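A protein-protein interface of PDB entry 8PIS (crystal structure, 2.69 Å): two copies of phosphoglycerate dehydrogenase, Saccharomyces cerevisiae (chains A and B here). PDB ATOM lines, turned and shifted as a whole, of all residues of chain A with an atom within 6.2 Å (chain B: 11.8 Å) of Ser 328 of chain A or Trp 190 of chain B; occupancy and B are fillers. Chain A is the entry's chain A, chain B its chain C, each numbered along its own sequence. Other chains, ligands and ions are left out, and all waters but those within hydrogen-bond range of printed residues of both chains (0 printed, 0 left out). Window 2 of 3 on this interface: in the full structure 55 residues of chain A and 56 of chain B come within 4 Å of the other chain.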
ATOM      1  N   ASP A 315      11.149 -20.308  21.735  1.00  0.00           N
ATOM      2  CA  ASP A 315      11.137 -19.963  20.322  1.00  0.00           C
ATOM      3  C   ASP A 315      12.217 -20.701  19.538  1.00  0.00           C
ATOM      4  O   ASP A 315      12.088 -20.852  18.319  1.00  0.00           O
ATOM      5  CB  ASP A 315      11.288 -18.434  20.173  1.00  0.00           C
ATOM      6  CG  ASP A 315      11.157 -17.940  18.723  1.00  0.00           C
ATOM      7  OD1 ASP A 315      10.044 -17.992  18.156  1.00  0.00           O
ATOM      8  OD2 ASP A 315      12.156 -17.416  18.178  1.00  0.00           O
ATOM      9  N   VAL A 316      13.242 -21.211  20.211  1.00  0.00           N
ATOM     10  CA  VAL A 316      14.362 -21.870  19.559  1.00  0.00           C
ATOM     11  C   VAL A 316      14.579 -23.222  20.215  1.00  0.00           C
ATOM     12  O   VAL A 316      14.195 -23.453  21.363  1.00  0.00           O
ATOM     13  CB  VAL A 316      15.642 -21.010  19.605  1.00  0.00           C
ATOM     14  CG1 VAL A 316      15.446 -19.780  18.779  1.00  0.00           C
ATOM     15  CG2 VAL A 316      15.924 -20.592  21.016  1.00  0.00           C
ATOM     16  N   TYR A 317      15.214 -24.122  19.474  1.00  0.00           N
ATOM     17  CA  TYR A 317      15.236 -25.523  19.859  1.00  0.00           C
ATOM     18  C   TYR A 317      16.582 -26.103  19.459  1.00  0.00           C
ATOM     19  O   TYR A 317      17.233 -25.569  18.553  1.00  0.00           O
ATOM     20  CB  TYR A 317      14.093 -26.279  19.170  1.00  0.00           C
ATOM     21  CG  TYR A 317      12.744 -25.676  19.483  1.00  0.00           C
ATOM     22  CD1 TYR A 317      12.104 -25.928  20.683  1.00  0.00           C
ATOM     23  CD2 TYR A 317      12.129 -24.825  18.574  1.00  0.00           C
ATOM     24  CE1 TYR A 317      10.872 -25.351  20.965  1.00  0.00           C
ATOM     25  CE2 TYR A 317      10.917 -24.249  18.838  1.00  0.00           C
ATOM     26  CZ  TYR A 317      10.286 -24.510  20.031  1.00  0.00           C
ATOM     27  OH  TYR A 317       9.064 -23.919  20.271  1.00  0.00           O
ATOM     28  N   HIS A 319      17.248 -28.780  17.753  1.00  0.00           N
ATOM     29  CA  HIS A 319      17.130 -29.202  16.361  1.00  0.00           C
ATOM     30  C   HIS A 319      15.848 -28.616  15.781  1.00  0.00           C
ATOM     31  O   HIS A 319      14.790 -28.695  16.413  1.00  0.00           O
ATOM     32  CB  HIS A 319      17.120 -30.735  16.248  1.00  0.00           C
ATOM     33  CG  HIS A 319      18.365 -31.393  16.763  1.00  0.00           C
ATOM     34  ND1 HIS A 319      19.557 -31.382  16.071  1.00  0.00           N
ATOM     35  CD2 HIS A 319      18.600 -32.082  17.905  1.00  0.00           C
ATOM     36  CE1 HIS A 319      20.474 -32.032  16.767  1.00  0.00           C
ATOM     37  NE2 HIS A 319      19.919 -32.465  17.884  1.00  0.00           N
ATOM     38  N   GLU A 320      15.941 -28.005  14.603  1.00  0.00           N
ATOM     39  CA  GLU A 320      14.777 -27.363  14.012  1.00  0.00           C
ATOM     40  C   GLU A 320      14.643 -27.803  12.560  1.00  0.00           C
ATOM     41  O   GLU A 320      15.649 -28.104  11.914  1.00  0.00           O
ATOM     42  CB  GLU A 320      14.900 -25.830  14.078  1.00  0.00           C
ATOM     43  CG  GLU A 320      15.056 -25.294  15.490  1.00  0.00           C
ATOM     44  CD  GLU A 320      15.180 -23.780  15.565  1.00  0.00           C
ATOM     45  OE1 GLU A 320      15.141 -23.109  14.511  1.00  0.00           O
ATOM     46  OE2 GLU A 320      15.382 -23.266  16.685  1.00  0.00           O
ATOM     47  N   PRO A 321      13.419 -27.882  12.030  1.00  0.00           N
ATOM     48  CA  PRO A 321      13.251 -28.283  10.629  1.00  0.00           C
ATOM     49  C   PRO A 321      13.857 -27.248   9.694  1.00  0.00           C
ATOM     50  O   PRO A 321      13.964 -26.064  10.024  1.00  0.00           O
ATOM     51  CB  PRO A 321      11.727 -28.353  10.455  1.00  0.00           C
ATOM     52  CG  PRO A 321      11.178 -28.486  11.845  1.00  0.00           C
ATOM     53  CD  PRO A 321      12.121 -27.675  12.694  1.00  0.00           C
ATOM     54  N   LYS A 323      12.484 -26.659   6.636  1.00  0.00           N
ATOM     55  CA  LYS A 323      11.392 -26.062   5.885  1.00  0.00           C
ATOM     56  C   LYS A 323      10.094 -26.248   6.654  1.00  0.00           C
ATOM     57  O   LYS A 323       9.976 -27.116   7.524  1.00  0.00           O
ATOM     58  CB  LYS A 323      11.267 -26.671   4.480  1.00  0.00           C
ATOM     59  N   ASN A 324       9.116 -25.405   6.332  1.00  0.00           N
ATOM     60  CA  ASN A 324       7.820 -25.500   6.985  1.00  0.00           C
ATOM     61  C   ASN A 324       7.057 -26.727   6.500  1.00  0.00           C
ATOM     62  O   ASN A 324       7.156 -27.121   5.335  1.00  0.00           O
ATOM     63  CB  ASN A 324       6.982 -24.250   6.724  1.00  0.00           C
ATOM     64  CG  ASN A 324       7.537 -23.024   7.401  1.00  0.00           C
ATOM     65  OD1 ASN A 324       8.076 -23.097   8.510  1.00  0.00           O
ATOM     66  ND2 ASN A 324       7.352 -21.875   6.770  1.00  0.00           N
ATOM     67  N   GLY A 325       6.317 -27.351   7.412  1.00  0.00           N
ATOM     68  CA  GLY A 325       5.483 -28.467   7.030  1.00  0.00           C
ATOM     69  C   GLY A 325       4.833 -29.162   8.204  1.00  0.00           C
ATOM     70  O   GLY A 325       5.245 -28.976   9.352  1.00  0.00           O
ATOM     71  N   GLU A 326       3.808 -29.959   7.925  1.00  0.00           N
ATOM     72  CA  GLU A 326       3.132 -30.716   8.962  1.00  0.00           C
ATOM     73  C   GLU A 326       3.991 -31.908   9.375  1.00  0.00           C
ATOM     74  O   GLU A 326       4.816 -32.401   8.601  1.00  0.00           O
ATOM     75  CB  GLU A 326       1.761 -31.176   8.472  1.00  0.00           C
ATOM     76  CG  GLU A 326       0.780 -30.033   8.258  1.00  0.00           C
ATOM     77  CD  GLU A 326      -0.576 -30.508   7.781  1.00  0.00           C
ATOM     78  OE1 GLU A 326      -0.710 -31.710   7.468  1.00  0.00           O
ATOM     79  OE2 GLU A 326      -1.514 -29.684   7.735  1.00  0.00           O
ATOM     80  N   GLY A 327       3.812 -32.359  10.617  1.00  0.00           N
ATOM     81  CA  GLY A 327       4.616 -33.457  11.116  1.00  0.00           C
ATOM     82  C   GLY A 327       6.094 -33.167  11.267  1.00  0.00           C
ATOM     83  O   GLY A 327       6.871 -34.102  11.464  1.00  0.00           O
ATOM     84  N   SER A 328       6.522 -31.909  11.119  1.00  0.00           N
ATOM     85  CA  SER A 328       7.946 -31.590  11.136  1.00  0.00           C
ATOM     86  C   SER A 328       8.526 -31.491  12.544  1.00  0.00           C
ATOM     87  O   SER A 328       9.750 -31.542  12.699  1.00  0.00           O
ATOM     88  CB  SER A 328       8.210 -30.278  10.388  1.00  0.00           C
ATOM     89  OG  SER A 328       7.912 -30.396   9.005  1.00  0.00           O
ATOM     90  N   PHE A 329       7.690 -31.326  13.568  1.00  0.00           N
ATOM     91  CA  PHE A 329       8.150 -31.039  14.928  1.00  0.00           C
ATOM     92  C   PHE A 329       7.726 -32.196  15.830  1.00  0.00           C
ATOM     93  O   PHE A 329       6.585 -32.238  16.297  1.00  0.00           O
ATOM     94  CB  PHE A 329       7.569 -29.700  15.388  1.00  0.00           C
ATOM     95  CG  PHE A 329       8.108 -29.203  16.698  1.00  0.00           C
ATOM     96  CD1 PHE A 329       9.363 -28.624  16.765  1.00  0.00           C
ATOM     97  CD2 PHE A 329       7.347 -29.279  17.855  1.00  0.00           C
ATOM     98  CE1 PHE A 329       9.865 -28.154  17.963  1.00  0.00           C
ATOM     99  CE2 PHE A 329       7.844 -28.809  19.058  1.00  0.00           C
ATOM    100  CZ  PHE A 329       9.103 -28.248  19.113  1.00  0.00           C
ATOM    101  N   ASN A 330       8.626 -33.141  16.074  1.00  0.00           N
ATOM    102  CA  ASN A 330       8.236 -34.389  16.720  1.00  0.00           C
ATOM    103  C   ASN A 330       9.465 -35.029  17.357  1.00  0.00           C
ATOM    104  O   ASN A 330      10.556 -34.449  17.365  1.00  0.00           O
ATOM    105  CB  ASN A 330       7.549 -35.323  15.721  1.00  0.00           C
ATOM    106  CG  ASN A 330       8.454 -35.730  14.575  1.00  0.00           C
ATOM    107  OD1 ASN A 330       9.650 -35.435  14.567  1.00  0.00           O
ATOM    108  ND2 ASN A 330       7.879 -36.401  13.588  1.00  0.00           N
ATOM    109  N   GLU A 332      11.362 -37.406  16.418  1.00  0.00           N
ATOM    110  CA  GLU A 332      12.519 -37.637  15.559  1.00  0.00           C
ATOM    111  C   GLU A 332      13.418 -36.411  15.511  1.00  0.00           C
ATOM    112  O   GLU A 332      14.643 -36.536  15.408  1.00  0.00           O
ATOM    113  CB  GLU A 332      12.070 -38.030  14.153  1.00  0.00           C
ATOM    114  CG  GLU A 332      13.197 -38.545  13.279  1.00  0.00           C
ATOM    115  CD  GLU A 332      13.975 -37.448  12.561  1.00  0.00           C
ATOM    116  OE1 GLU A 332      13.377 -36.404  12.225  1.00  0.00           O
ATOM    117  OE2 GLU A 332      15.194 -37.629  12.349  1.00  0.00           O
ATOM    118  N   LEU A 333      12.827 -35.221  15.600  1.00  0.00           N
ATOM    119  CA  LEU A 333      13.601 -33.989  15.631  1.00  0.00           C
ATOM    120  C   LEU A 333      14.203 -33.747  17.011  1.00  0.00           C
ATOM    121  O   LEU A 333      15.388 -33.417  17.132  1.00  0.00           O
ATOM    122  CB  LEU A 333      12.705 -32.827  15.209  1.00  0.00           C
ATOM    123  CG  LEU A 333      13.325 -31.443  15.076  1.00  0.00           C
ATOM    124  CD1 LEU A 333      14.393 -31.487  14.026  1.00  0.00           C
ATOM    125  CD2 LEU A 333      12.241 -30.439  14.706  1.00  0.00           C
ATOM    126  N   THR A 349       6.999 -21.653  19.773  1.00  0.00           N
ATOM    127  CA  THR A 349       6.892 -20.911  18.533  1.00  0.00           C
ATOM    128  C   THR A 349       7.984 -21.343  17.567  1.00  0.00           C
ATOM    129  O   THR A 349       9.104 -21.658  17.986  1.00  0.00           O
ATOM    130  CB  THR A 349       6.962 -19.389  18.774  1.00  0.00           C
ATOM    131  OG1 THR A 349       8.168 -19.046  19.464  1.00  0.00           O
ATOM    132  CG2 THR A 349       5.754 -18.911  19.565  1.00  0.00           C
ATOM    133  N   PRO A 350       7.680 -21.396  16.276  1.00  0.00           N
ATOM    134  CA  PRO A 350       8.647 -21.911  15.294  1.00  0.00           C
ATOM    135  C   PRO A 350       9.692 -20.869  14.901  1.00  0.00           C
ATOM    136  O   PRO A 350       9.812 -20.483  13.737  1.00  0.00           O
ATOM    137  CB  PRO A 350       7.742 -22.310  14.121  1.00  0.00           C
ATOM    138  CG  PRO A 350       6.590 -21.390  14.206  1.00  0.00           C
ATOM    139  CD  PRO A 350       6.354 -21.156  15.675  1.00  0.00           C
ATOM    140  N   HIS A 351      10.432 -20.377  15.900  1.00  0.00           N
ATOM    141  CA  HIS A 351      11.579 -19.483  15.688  1.00  0.00           C
ATOM    142  C   HIS A 351      11.168 -18.223  14.924  1.00  0.00           C
ATOM    143  O   HIS A 351      11.800 -17.819  13.948  1.00  0.00           O
ATOM    144  CB  HIS A 351      12.723 -20.247  15.000  1.00  0.00           C
ATOM    145  CG  HIS A 351      14.051 -19.553  15.046  1.00  0.00           C
ATOM    146  ND1 HIS A 351      15.189 -20.094  14.480  1.00  0.00           N
ATOM    147  CD2 HIS A 351      14.421 -18.352  15.550  1.00  0.00           C
ATOM    148  CE1 HIS A 351      16.208 -19.275  14.673  1.00  0.00           C
ATOM    149  NE2 HIS A 351      15.768 -18.206  15.311  1.00  0.00           N
ATOM    150  N   GLN B 177       0.561 -13.750  15.676  1.00  0.00           N
ATOM    151  CA  GLN B 177      -0.113 -15.049  15.533  1.00  0.00           C
ATOM    152  C   GLN B 177       0.447 -16.107  16.491  1.00  0.00           C
ATOM    153  O   GLN B 177       0.550 -17.285  16.150  1.00  0.00           O
ATOM    154  CB  GLN B 177      -0.049 -15.536  14.081  1.00  0.00           C
ATOM    155  CG  GLN B 177      -0.757 -14.617  13.106  1.00  0.00           C
ATOM    156  CD  GLN B 177      -0.589 -15.049  11.663  1.00  0.00           C
ATOM    157  OE1 GLN B 177       0.028 -16.071  11.372  1.00  0.00           O
ATOM    158  NE2 GLN B 177      -1.110 -14.247  10.747  1.00  0.00           N
ATOM    159  N   LEU B 178       0.749 -15.698  17.725  1.00  0.00           N
ATOM    160  CA  LEU B 178       1.332 -16.622  18.695  1.00  0.00           C
ATOM    161  C   LEU B 178       0.408 -17.790  18.972  1.00  0.00           C
ATOM    162  O   LEU B 178       0.855 -18.943  19.034  1.00  0.00           O
ATOM    163  CB  LEU B 178       1.635 -15.904  20.004  1.00  0.00           C
ATOM    164  CG  LEU B 178       2.708 -14.832  19.959  1.00  0.00           C
ATOM    165  CD1 LEU B 178       2.828 -14.153  21.329  1.00  0.00           C
ATOM    166  CD2 LEU B 178       4.003 -15.475  19.533  1.00  0.00           C
ATOM    167  N   GLY B 179      -0.879 -17.504  19.191  1.00  0.00           N
ATOM    168  CA  GLY B 179      -1.834 -18.567  19.452  1.00  0.00           C
ATOM    169  C   GLY B 179      -1.788 -19.658  18.404  1.00  0.00           C
ATOM    170  O   GLY B 179      -1.680 -20.844  18.725  1.00  0.00           O
ATOM    171  N   ASP B 180      -1.851 -19.275  17.130  1.00  0.00           N
ATOM    172  CA  ASP B 180      -1.821 -20.280  16.076  1.00  0.00           C
ATOM    173  C   ASP B 180      -0.487 -21.009  16.054  1.00  0.00           C
ATOM    174  O   ASP B 180      -0.453 -22.238  15.968  1.00  0.00           O
ATOM    175  CB  ASP B 180      -2.129 -19.661  14.713  1.00  0.00           C
ATOM    176  CG  ASP B 180      -3.592 -19.283  14.566  1.00  0.00           C
ATOM    177  OD1 ASP B 180      -4.431 -19.852  15.298  1.00  0.00           O
ATOM    178  OD2 ASP B 180      -3.908 -18.442  13.699  1.00  0.00           O
ATOM    179  N   ARG B 181       0.624 -20.269  16.105  1.00  0.00           N
ATOM    180  CA  ARG B 181       1.935 -20.908  16.057  1.00  0.00           C
ATOM    181  C   ARG B 181       2.071 -21.980  17.131  1.00  0.00           C
ATOM    182  O   ARG B 181       2.572 -23.079  16.865  1.00  0.00           O
ATOM    183  CB  ARG B 181       3.049 -19.872  16.217  1.00  0.00           C
ATOM    184  CG  ARG B 181       3.109 -18.792  15.151  1.00  0.00           C
ATOM    185  CD  ARG B 181       3.530 -19.315  13.784  1.00  0.00           C
ATOM    186  NE  ARG B 181       2.399 -19.863  13.040  1.00  0.00           N
ATOM    187  CZ  ARG B 181       1.500 -19.119  12.395  1.00  0.00           C
ATOM    188  NH1 ARG B 181       1.607 -17.796  12.390  1.00  0.00           N
ATOM    189  NH2 ARG B 181       0.493 -19.692  11.746  1.00  0.00           N
ATOM    190  N   SER B 182       1.614 -21.686  18.349  1.00  0.00           N
ATOM    191  CA  SER B 182       1.818 -22.628  19.444  1.00  0.00           C
ATOM    192  C   SER B 182       0.882 -23.821  19.342  1.00  0.00           C
ATOM    193  O   SER B 182       1.270 -24.943  19.682  1.00  0.00           O
ATOM    194  CB  SER B 182       1.659 -21.923  20.789  1.00  0.00           C
ATOM    195  OG  SER B 182       1.909 -22.814  21.858  1.00  0.00           O
ATOM    196  N   ILE B 183      -0.355 -23.606  18.894  1.00  0.00           N
ATOM    197  CA  ILE B 183      -1.232 -24.737  18.620  1.00  0.00           C
ATOM    198  C   ILE B 183      -0.613 -25.620  17.551  1.00  0.00           C
ATOM    199  O   ILE B 183      -0.700 -26.853  17.605  1.00  0.00           O
ATOM    200  CB  ILE B 183      -2.629 -24.236  18.206  1.00  0.00           C
ATOM    201  CG1 ILE B 183      -3.277 -23.459  19.349  1.00  0.00           C
ATOM    202  CG2 ILE B 183      -3.526 -25.398  17.780  1.00  0.00           C
ATOM    203  CD1 ILE B 183      -4.492 -22.658  18.911  1.00  0.00           C
ATOM    204  N   GLU B 184       0.046 -24.999  16.575  1.00  0.00           N
ATOM    205  CA  GLU B 184       0.668 -25.749  15.492  1.00  0.00           C
ATOM    206  C   GLU B 184       1.805 -26.628  16.003  1.00  0.00           C
ATOM    207  O   GLU B 184       1.844 -27.832  15.720  1.00  0.00           O
ATOM    208  CB  GLU B 184       1.137 -24.767  14.412  1.00  0.00           C
ATOM    209  CG  GLU B 184      -0.031 -24.051  13.698  1.00  0.00           C
ATOM    210  CD  GLU B 184       0.412 -22.890  12.802  1.00  0.00           C
ATOM    211  OE1 GLU B 184       1.612 -22.544  12.797  1.00  0.00           O
ATOM    212  OE2 GLU B 184      -0.452 -22.309  12.114  1.00  0.00           O
ATOM    213  N   LEU B 185       2.714 -26.066  16.804  1.00  0.00           N
ATOM    214  CA  LEU B 185       3.820 -26.893  17.294  1.00  0.00           C
ATOM    215  C   LEU B 185       3.330 -27.952  18.265  1.00  0.00           C
ATOM    216  O   LEU B 185       3.831 -29.082  18.252  1.00  0.00           O
ATOM    217  CB  LEU B 185       4.907 -26.049  17.947  1.00  0.00           C
ATOM    218  CG  LEU B 185       5.811 -25.245  17.022  1.00  0.00           C
ATOM    219  CD1 LEU B 185       6.919 -24.625  17.848  1.00  0.00           C
ATOM    220  CD2 LEU B 185       6.383 -26.121  15.929  1.00  0.00           C
ATOM    221  N   HIS B 186       2.331 -27.632  19.092  1.00  0.00           N
ATOM    222  CA  HIS B 186       1.781 -28.659  19.968  1.00  0.00           C
ATOM    223  C   HIS B 186       1.179 -29.823  19.193  1.00  0.00           C
ATOM    224  O   HIS B 186       0.903 -30.866  19.793  1.00  0.00           O
ATOM    225  CB  HIS B 186       0.729 -28.072  20.913  1.00  0.00           C
ATOM    226  CG  HIS B 186       1.295 -27.351  22.097  1.00  0.00           C
ATOM    227  ND1 HIS B 186       1.696 -26.034  22.052  1.00  0.00           N
ATOM    228  CD2 HIS B 186       1.477 -27.755  23.377  1.00  0.00           C
ATOM    229  CE1 HIS B 186       2.128 -25.664  23.245  1.00  0.00           C
ATOM    230  NE2 HIS B 186       2.005 -26.690  24.068  1.00  0.00           N
ATOM    231  N   THR B 187       0.954 -29.681  17.888  1.00  0.00           N
ATOM    232  CA  THR B 187       0.505 -30.802  17.074  1.00  0.00           C
ATOM    233  C   THR B 187       1.492 -31.146  15.964  1.00  0.00           C
ATOM    234  O   THR B 187       1.124 -31.835  15.008  1.00  0.00           O
ATOM    235  CB  THR B 187      -0.882 -30.520  16.501  1.00  0.00           C
ATOM    236  OG1 THR B 187      -0.822 -29.375  15.644  1.00  0.00           O
ATOM    237  CG2 THR B 187      -1.868 -30.243  17.638  1.00  0.00           C
ATOM    238  N   GLY B 188       2.751 -30.700  16.076  1.00  0.00           N
ATOM    239  CA  GLY B 188       3.794 -31.111  15.158  1.00  0.00           C
ATOM    240  C   GLY B 188       4.051 -30.194  13.981  1.00  0.00           C
ATOM    241  O   GLY B 188       5.052 -30.387  13.270  1.00  0.00           O
ATOM    242  N   THR B 189       3.181 -29.225  13.725  1.00  0.00           N
ATOM    243  CA  THR B 189       3.331 -28.383  12.549  1.00  0.00           C
ATOM    244  C   THR B 189       4.341 -27.272  12.824  1.00  0.00           C
ATOM    245  O   THR B 189       4.228 -26.550  13.818  1.00  0.00           O
ATOM    246  CB  THR B 189       1.979 -27.788  12.138  1.00  0.00           C
ATOM    247  OG1 THR B 189       1.052 -28.843  11.864  1.00  0.00           O
ATOM    248  CG2 THR B 189       2.130 -26.933  10.893  1.00  0.00           C
ATOM    249  N   TRP B 190       5.340 -27.156  11.955  1.00  0.00           N
ATOM    250  CA  TRP B 190       6.317 -26.073  11.998  1.00  0.00           C
ATOM    251  C   TRP B 190       5.941 -25.063  10.925  1.00  0.00           C
ATOM    252  O   TRP B 190       6.035 -25.366   9.732  1.00  0.00           O
ATOM    253  CB  TRP B 190       7.732 -26.588  11.738  1.00  0.00           C
ATOM    254  CG  TRP B 190       8.784 -25.518  11.869  1.00  0.00           C
ATOM    255  CD1 TRP B 190       9.227 -24.674  10.886  1.00  0.00           C
ATOM    256  CD2 TRP B 190       9.574 -25.229  13.027  1.00  0.00           C
ATOM    257  NE1 TRP B 190      10.212 -23.848  11.376  1.00  0.00           N
ATOM    258  CE2 TRP B 190      10.447 -24.173  12.687  1.00  0.00           C
ATOM    259  CE3 TRP B 190       9.622 -25.750  14.325  1.00  0.00           C
ATOM    260  CZ2 TRP B 190      11.355 -23.632  13.599  1.00  0.00           C
ATOM    261  CZ3 TRP B 190      10.526 -25.209  15.229  1.00  0.00           C
ATOM    262  CH2 TRP B 190      11.380 -24.165  14.862  1.00  0.00           C
ATOM    263  N   ASN B 191       5.566 -23.852  11.340  1.00  0.00           N
ATOM    264  CA  ASN B 191       5.042 -22.863  10.401  1.00  0.00           C
ATOM    265  C   ASN B 191       5.584 -21.473  10.762  1.00  0.00           C
ATOM    266  O   ASN B 191       4.868 -20.624  11.306  1.00  0.00           O
ATOM    267  CB  ASN B 191       3.518 -22.885  10.407  1.00  0.00           C
ATOM    268  CG  ASN B 191       2.921 -22.178   9.221  1.00  0.00           C
ATOM    269  OD1 ASN B 191       3.629 -21.739   8.328  1.00  0.00           O
ATOM    270  ND2 ASN B 191       1.604 -22.045   9.218  1.00  0.00           N
ATOM    271  N   LYS B 192       6.855 -21.235  10.427  1.00  0.00           N
ATOM    272  CA  LYS B 192       7.449 -19.914  10.596  1.00  0.00           C
ATOM    273  C   LYS B 192       6.822 -18.951   9.592  1.00  0.00           C
ATOM    274  O   LYS B 192       6.957 -19.138   8.379  1.00  0.00           O
ATOM    275  CB  LYS B 192       8.962 -19.975  10.408  1.00  0.00           C
ATOM    276  CG  LYS B 192       9.674 -18.655  10.700  1.00  0.00           C
ATOM    277  CD  LYS B 192      11.172 -18.696  10.344  1.00  0.00           C
ATOM    278  CE  LYS B 192      11.987 -19.500  11.352  1.00  0.00           C
ATOM    279  NZ  LYS B 192      13.474 -19.425  11.129  1.00  0.00           N
ATOM    280  N   VAL B 193       6.126 -17.930  10.091  1.00  0.00           N
ATOM    281  CA  VAL B 193       5.411 -16.976   9.249  1.00  0.00           C
ATOM    282  C   VAL B 193       5.836 -15.563   9.625  1.00  0.00           C
ATOM    283  O   VAL B 193       5.683 -15.149  10.782  1.00  0.00           O
ATOM    284  CB  VAL B 193       3.886 -17.120   9.394  1.00  0.00           C
ATOM    285  CG1 VAL B 193       3.172 -15.995   8.652  1.00  0.00           C
ATOM    286  CG2 VAL B 193       3.426 -18.477   8.889  1.00  0.00           C
ATOM    287  N   ALA B 194       6.341 -14.813   8.646  1.00  0.00           N
ATOM    288  CA  ALA B 194       6.533 -13.383   8.813  1.00  0.00           C
ATOM    289  C   ALA B 194       5.527 -12.551   8.024  1.00  0.00           C
ATOM    290  O   ALA B 194       5.382 -11.359   8.305  1.00  0.00           O
ATOM    291  CB  ALA B 194       7.958 -12.976   8.417  1.00  0.00           C
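No position is printed for both chains.
Among the printed residues, pairs that only touch across the chains: His 351 of chain A with Lys 192 of chain B, Tyr 317 of chain A with Leu 185 of chain B, Pro 350 of chain A with Lys 192 of chain B, Pro 350 of chain A with Asn 191 of chain B, Thr 349 of chain A with Leu 185 of chain B, Pro 350 of chain A with Trp 190 of chain B, Gly 327 of chain A with Gly 188 of chain B, Phe 329 of chain A with Leu 185 of chain B, Pro 321 of chain A with Trp 190 of chain B, Asn 324 of chain A with Asn 191 of chain B, Pro 350 of chain A with Arg 181 of chain B, Pro 350 of chain A with Leu 185 of chain B, Tyr 317 of chain A with Trp 190 of chain B, Gly 325 of chain A with Thr 189 of chain B, Phe 329 of chain A with Trp 190 of chain B, Glu 326 of chain A with Thr 189 of chain B, Thr 349 of chain A with Leu 178 of chain B, Glu 320 of chain A with Trp 190 of chain B, His 351 of chain A with Trp 190 of chain B and Ser 328 of chain A with Trp 190 of chain B.
Of chain B, only Leu 185 (3.3 Å) and Trp 190 (3.7 Å) come within 4 Å of Tyr 317 of chain A.
Of chain B, only Trp 190 (3.5 Å) comes within 4 Å of Pro 321 of chain A.
No residue of chain B comes within 4 Å of Lys 323 of chain A.
Of the printed residues of chain B, Gly 325 of chain A touches Thr 189 (3.8 Å) and Trp 190 (3.1 Å).
Of the printed residues of chain B, Gly 327 of chain A touches Gly 188.
Ser 328 of chain A touches two residues of chain B.
Phe 329 of chain A touches just these residues of chain B: Leu 185, Gly 188 and Trp 190.
No residue of chain B comes within 4 Å of Asn 330 of chain A.
No residue of chain B comes within 4 Å of Leu 333 of chain A.
Of the printed residues of chain B, Thr 349 of chain A touches Leu 178 (3.9 Å) and Leu 185 (3.5 Å).
Of the printed residues of chain B, His 351 of chain A touches Trp 190 and Lys 192.
Ser 182 of chain B touches none of the printed residues of chain A.
His 186 of chain B touches none of the printed residues of chain A.
Of chain A, only Tyr 317 (3.7 Å), Glu 320 (3.9 Å), Pro 321 (3.5 Å), Asn 324 (3.1 Å), Gly 325 (3.1 Å), Ser 328 (3.96 Å), Phe 329 (3.8 Å), Pro 350 (3.5 Å) and His 351 (3.9 Å) come within 4 Å of Trp 190 of chain B.
Printed residues of chain A within 4 Å of Lys 192 of chain B: Asn 324, Pro 350 and His 351.
The nearest residue of chain B that does not touch Ser 328 of chain A is Thr 189 of chain B (5.0 Å).
The nearest residue of chain A that does not touch Trp 190 of chain B is Lys 323 of chain A (4.2 Å).
The nearest printed residue of chain A that does not touch Leu 178 of chain B is Asp 315 of chain A (6.7 Å).
The side-chain hydroxyl of Thr 349 of chain A is in hydrogen-bond range of the side-chain carboxylate of Asp 315 of chain A, at 2.5 Å.
The backbone NH (N) of Thr 349 of chain A is in hydrogen-bond range of the side-chain hydroxyl (OH) of Tyr 317 of chain A (3.1 Å).
The backbone carbonyl oxygen (O) of Gly 325 of chain A is in hydrogen-bond range of the side-chain hydroxyl (OG) of Ser 328 of chain A (3.0 Å).
ND2 of Asn 330 of chain A sits at hydrogen-bond distance from O of Gly 327 of chain A (3.3 Å).
The backbone carbonyl oxygen (O) of Glu 184 of chain B is in hydrogen-bond range of the backbone NH (N) of Thr 189 of chain B, 2.8 Å away.
Printed residues of chain A that touch a printed residue of chain B: Tyr 317, Glu 320, Pro 321, Asn 324, Gly 325, Glu 326, Gly 327, Ser 328, Phe 329, Thr 349, Pro 350 and His 351.
Hydrophobic or aromatic side chains of chain A that line the printed part of chain B: Tyr 317, Pro 321, Phe 329, Pro 350 and His 351.
Hydrophobic or aromatic side chains of chain B that line the printed part of chain A: Leu 178, Leu 185 and Trp 190.
Among the printed residues, no Asp or Glu carboxylate lies within 4 Å of a Lys or Arg side-chain nitrogen of the other chain.
The side-chain amide oxygen of Asn 324 of chain A lies close to the backbone carbonyl oxygen of Trp 190 of chain B, 3.3 Å away.
N of Lys 192 of chain B sits at hydrogen-bond distance from OD1 of Asn 324 of chain A, at 2.9 Å.
The backbone NH (N) of Gly 325 of chain A lies within hydrogen-bond range of the backbone carbonyl oxygen (O) of Trp 190 of chain B (3.1 Å).
N of Ser 328 of chain A sits at hydrogen-bond distance from O of Gly 188 of chain B, at 3.0 Å.
N of Phe 329 of chain A lies within hydrogen-bond range of O of Gly 188 of chain B, at 2.8 Å.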
